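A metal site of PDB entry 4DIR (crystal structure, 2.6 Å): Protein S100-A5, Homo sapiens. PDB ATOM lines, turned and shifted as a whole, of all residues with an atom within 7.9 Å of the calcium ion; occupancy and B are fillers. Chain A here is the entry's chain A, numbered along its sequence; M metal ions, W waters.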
ATOM      1  N   THR A  28      21.372  18.372   9.644  1.00  0.00           N
ATOM      2  CA  THR A  28      21.585  19.261  10.764  1.00  0.00           C
ATOM      3  C   THR A  28      22.784  18.823  11.604  1.00  0.00           C
ATOM      4  O   THR A  28      23.203  17.666  11.589  1.00  0.00           O
ATOM      5  CB  THR A  28      20.391  19.321  11.699  1.00  0.00           C
ATOM      6  OG1 THR A  28      20.285  18.047  12.333  1.00  0.00           O
ATOM      7  CG2 THR A  28      19.074  19.745  10.972  1.00  0.00           C
ATOM      8  N   LEU A  29      23.322  19.801  12.331  1.00  0.00           N
ATOM      9  CA  LEU A  29      24.448  19.609  13.243  1.00  0.00           C
ATOM     10  C   LEU A  29      23.875  19.476  14.625  1.00  0.00           C
ATOM     11  O   LEU A  29      23.167  20.350  15.075  1.00  0.00           O
ATOM     12  CB  LEU A  29      25.372  20.818  13.219  1.00  0.00           C
ATOM     13  CG  LEU A  29      26.179  21.113  11.969  1.00  0.00           C
ATOM     14  CD1 LEU A  29      26.673  22.561  11.987  1.00  0.00           C
ATOM     15  CD2 LEU A  29      27.382  20.212  11.940  1.00  0.00           C
ATOM     16  N   MET A  56      25.315  27.380  20.792  1.00  0.00           N
ATOM     17  CA  MET A  56      24.041  26.672  20.607  1.00  0.00           C
ATOM     18  C   MET A  56      22.813  27.564  20.886  1.00  0.00           C
ATOM     19  O   MET A  56      21.913  27.684  20.066  1.00  0.00           O
ATOM     20  CB  MET A  56      24.031  25.492  21.562  1.00  0.00           C
ATOM     21  CG  MET A  56      23.421  24.250  21.008  1.00  0.00           C
ATOM     22  SD  MET A  56      24.071  23.767  19.387  1.00  0.00           S
ATOM     23  CE  MET A  56      22.892  22.424  19.074  1.00  0.00           C
ATOM     24  N   LEU A  59      22.528  30.269  18.168  1.00  0.00           N
ATOM     25  CA  LEU A  59      22.221  29.843  16.780  1.00  0.00           C
ATOM     26  C   LEU A  59      20.965  29.012  16.627  1.00  0.00           C
ATOM     27  O   LEU A  59      20.355  29.000  15.538  1.00  0.00           O
ATOM     28  CB  LEU A  59      23.351  28.960  16.228  1.00  0.00           C
ATOM     29  CG  LEU A  59      24.804  29.421  16.188  1.00  0.00           C
ATOM     30  CD1 LEU A  59      25.646  28.365  15.547  1.00  0.00           C
ATOM     31  CD2 LEU A  59      24.867  30.687  15.389  1.00  0.00           C
ATOM     32  N   ASP A  60      20.626  28.264  17.681  1.00  0.00           N
ATOM     33  CA  ASP A  60      19.486  27.390  17.609  1.00  0.00           C
ATOM     34  C   ASP A  60      18.182  28.153  17.682  1.00  0.00           C
ATOM     35  O   ASP A  60      17.551  28.188  18.715  1.00  0.00           O
ATOM     36  CB  ASP A  60      19.547  26.362  18.714  1.00  0.00           C
ATOM     37  CG  ASP A  60      18.539  25.265  18.521  1.00  0.00           C
ATOM     38  OD1 ASP A  60      18.075  25.088  17.378  1.00  0.00           O
ATOM     39  OD2 ASP A  60      18.191  24.571  19.489  1.00  0.00           O
ATOM     40  N   LYS A  61      17.757  28.750  16.577  1.00  0.00           N
ATOM     41  CA  LYS A  61      16.522  29.576  16.552  1.00  0.00           C
ATOM     42  C   LYS A  61      15.285  28.806  17.008  1.00  0.00           C
ATOM     43  O   LYS A  61      14.513  29.328  17.809  1.00  0.00           O
ATOM     44  CB  LYS A  61      16.285  30.233  15.173  1.00  0.00           C
ATOM     45  N   ASN A  62      15.098  27.568  16.532  1.00  0.00           N
ATOM     46  CA  ASN A  62      13.888  26.796  16.863  1.00  0.00           C
ATOM     47  C   ASN A  62      13.922  25.916  18.135  1.00  0.00           C
ATOM     48  O   ASN A  62      12.992  25.140  18.377  1.00  0.00           O
ATOM     49  CB  ASN A  62      13.392  25.983  15.657  1.00  0.00           C
ATOM     50  CG  ASN A  62      14.408  24.965  15.174  1.00  0.00           C
ATOM     51  OD1 ASN A  62      15.569  24.976  15.592  1.00  0.00           O
ATOM     52  ND2 ASN A  62      13.971  24.061  14.285  1.00  0.00           N
ATOM     53  N   SER A  63      14.987  26.028  18.948  1.00  0.00           N
ATOM     54  CA  SER A  63      15.083  25.299  20.218  1.00  0.00           C
ATOM     55  C   SER A  63      14.951  23.765  20.077  1.00  0.00           C
ATOM     56  O   SER A  63      14.628  23.046  21.055  1.00  0.00           O
ATOM     57  CB  SER A  63      14.073  25.850  21.238  1.00  0.00           C
ATOM     58  OG  SER A  63      14.541  27.081  21.733  1.00  0.00           O
ATOM     59  N   ASP A  64      15.230  23.262  18.872  1.00  0.00           N
ATOM     60  CA  ASP A  64      15.190  21.821  18.612  1.00  0.00           C
ATOM     61  C   ASP A  64      16.504  21.152  18.899  1.00  0.00           C
ATOM     62  O   ASP A  64      16.642  19.950  18.688  1.00  0.00           O
ATOM     63  CB  ASP A  64      14.743  21.504  17.164  1.00  0.00           C
ATOM     64  CG  ASP A  64      15.776  21.927  16.084  1.00  0.00           C
ATOM     65  OD1 ASP A  64      16.815  22.547  16.402  1.00  0.00           O
ATOM     66  OD2 ASP A  64      15.549  21.644  14.887  1.00  0.00           O
ATOM     67  N   GLN A  65      17.500  21.915  19.318  1.00  0.00           N
ATOM     68  CA  GLN A  65      18.790  21.371  19.718  1.00  0.00           C
ATOM     69  C   GLN A  65      19.623  20.848  18.581  1.00  0.00           C
ATOM     70  O   GLN A  65      20.474  20.017  18.766  1.00  0.00           O
ATOM     71  CB  GLN A  65      18.613  20.307  20.793  1.00  0.00           C
ATOM     72  CG  GLN A  65      18.089  20.835  22.138  1.00  0.00           C
ATOM     73  CD  GLN A  65      19.077  20.720  23.283  1.00  0.00           C
ATOM     74  OE1 GLN A  65      18.707  20.364  24.394  1.00  0.00           O
ATOM     75  NE2 GLN A  65      20.344  21.027  23.023  1.00  0.00           N
ATOM     76  N   GLU A  66      19.399  21.340  17.358  1.00  0.00           N
ATOM     77  CA  GLU A  66      20.172  20.974  16.186  1.00  0.00           C
ATOM     78  C   GLU A  66      20.368  22.208  15.396  1.00  0.00           C
ATOM     79  O   GLU A  66      19.513  23.076  15.403  1.00  0.00           O
ATOM     80  CB  GLU A  66      19.404  20.038  15.277  1.00  0.00           C
ATOM     81  CG  GLU A  66      18.863  18.801  15.896  1.00  0.00           C
ATOM     82  CD  GLU A  66      18.200  17.914  14.846  1.00  0.00           C
ATOM     83  OE1 GLU A  66      18.911  17.103  14.260  1.00  0.00           O
ATOM     84  OE2 GLU A  66      16.982  18.005  14.599  1.00  0.00           O
ATOM     85  N   ILE A  67      21.466  22.277  14.713  1.00  0.00           N
ATOM     86  CA  ILE A  67      21.754  23.424  13.887  1.00  0.00           C
ATOM     87  C   ILE A  67      21.461  23.085  12.416  1.00  0.00           C
ATOM     88  O   ILE A  67      22.195  22.316  11.781  1.00  0.00           O
ATOM     89  CB  ILE A  67      23.195  23.941  14.148  1.00  0.00           C
ATOM     90  CG1 ILE A  67      23.387  24.287  15.640  1.00  0.00           C
ATOM     91  CG2 ILE A  67      23.490  25.181  13.308  1.00  0.00           C
ATOM     92  CD1 ILE A  67      22.363  25.360  16.204  1.00  0.00           C
ATOM     93  N   ASP A  68      20.356  23.589  11.873  1.00  0.00           N
ATOM     94  CA  ASP A  68      20.106  23.347  10.443  1.00  0.00           C
ATOM     95  C   ASP A  68      20.983  24.286   9.609  1.00  0.00           C
ATOM     96  O   ASP A  68      21.675  25.137  10.167  1.00  0.00           O
ATOM     97  CB  ASP A  68      18.596  23.420  10.090  1.00  0.00           C
ATOM     98  CG  ASP A  68      18.029  24.833  10.100  1.00  0.00           C
ATOM     99  OD1 ASP A  68      18.820  25.788  10.071  1.00  0.00           O
ATOM    100  OD2 ASP A  68      16.800  25.016  10.126  1.00  0.00           O
ATOM    101  N   PHE A  69      20.946  24.156   8.278  1.00  0.00           N
ATOM    102  CA  PHE A  69      21.900  24.878   7.427  1.00  0.00           C
ATOM    103  C   PHE A  69      21.704  26.395   7.466  1.00  0.00           C
ATOM    104  O   PHE A  69      22.686  27.135   7.489  1.00  0.00           O
ATOM    105  CB  PHE A  69      21.907  24.353   5.981  1.00  0.00           C
ATOM    106  CG  PHE A  69      22.975  24.985   5.158  1.00  0.00           C
ATOM    107  CD1 PHE A  69      24.292  24.518   5.229  1.00  0.00           C
ATOM    108  CD2 PHE A  69      22.710  26.108   4.409  1.00  0.00           C
ATOM    109  CE1 PHE A  69      25.352  25.161   4.499  1.00  0.00           C
ATOM    110  CE2 PHE A  69      23.766  26.776   3.658  1.00  0.00           C
ATOM    111  CZ  PHE A  69      25.091  26.299   3.702  1.00  0.00           C
ATOM    112  N   GLU A  71      20.538  28.116  10.003  1.00  0.00           N
ATOM    113  CA  GLU A  71      21.048  28.526  11.323  1.00  0.00           C
ATOM    114  C   GLU A  71      22.583  28.592  11.330  1.00  0.00           C
ATOM    115  O   GLU A  71      23.160  29.488  11.907  1.00  0.00           O
ATOM    116  CB  GLU A  71      20.522  27.594  12.408  1.00  0.00           C
ATOM    117  CG  GLU A  71      19.012  27.704  12.621  1.00  0.00           C
ATOM    118  CD  GLU A  71      18.424  26.661  13.639  1.00  0.00           C
ATOM    119  OE1 GLU A  71      18.912  25.482  13.675  1.00  0.00           O
ATOM    120  OE2 GLU A  71      17.458  26.999  14.384  1.00  0.00           O
HETATM  121 CA    CA M   1      17.477  24.297  15.069  1.00  0.00          CA
HETATM  122  O   HOH W   1      16.728  23.795  12.749  1.00  0.00           O
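The side-chain carboxylate (OD1) of Asp 68 sits at hydrogen-bond distance from the backbone NH (N) of Glu 71. The backbone NH (N) of Lys 61 lies close to the side-chain carboxylate (OE2) of Glu 71 (2.8 Å). The side-chain carboxylate (OE1) of Glu 66 lies within hydrogen-bond range of the side-chain hydroxyl (OG1) of Thr 28 (2.5 Å). The backbone NH (N) of Gln 65 lies within hydrogen-bond range of the side-chain carboxylate (OD2) of Asp 60.
The calcium ion is bound by the side-chain amide oxygen (OD1) of Asn 62 (2.1 Å), the side-chain carboxylate (OD1) of Asp 64 (2.3 Å), the side-chain carboxylate (OE1) of Glu 71 (2.3 Å), the backbone carbonyl oxygen (O) of Glu 66 (2.4 Å), water W1 (2.5 Å), the side-chain carboxylate (OD1) of Asp 60 (2.5 Å) and the side-chain carboxylate (OE2) of Glu 71 (2.8 Å).
Water W1 lies within hydrogen-bond range of OD2 of Asp 68 (2.9 Å), ND2 of Asn 62 (3.2 Å) and OD2 of Asp 64 (3.3 Å).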
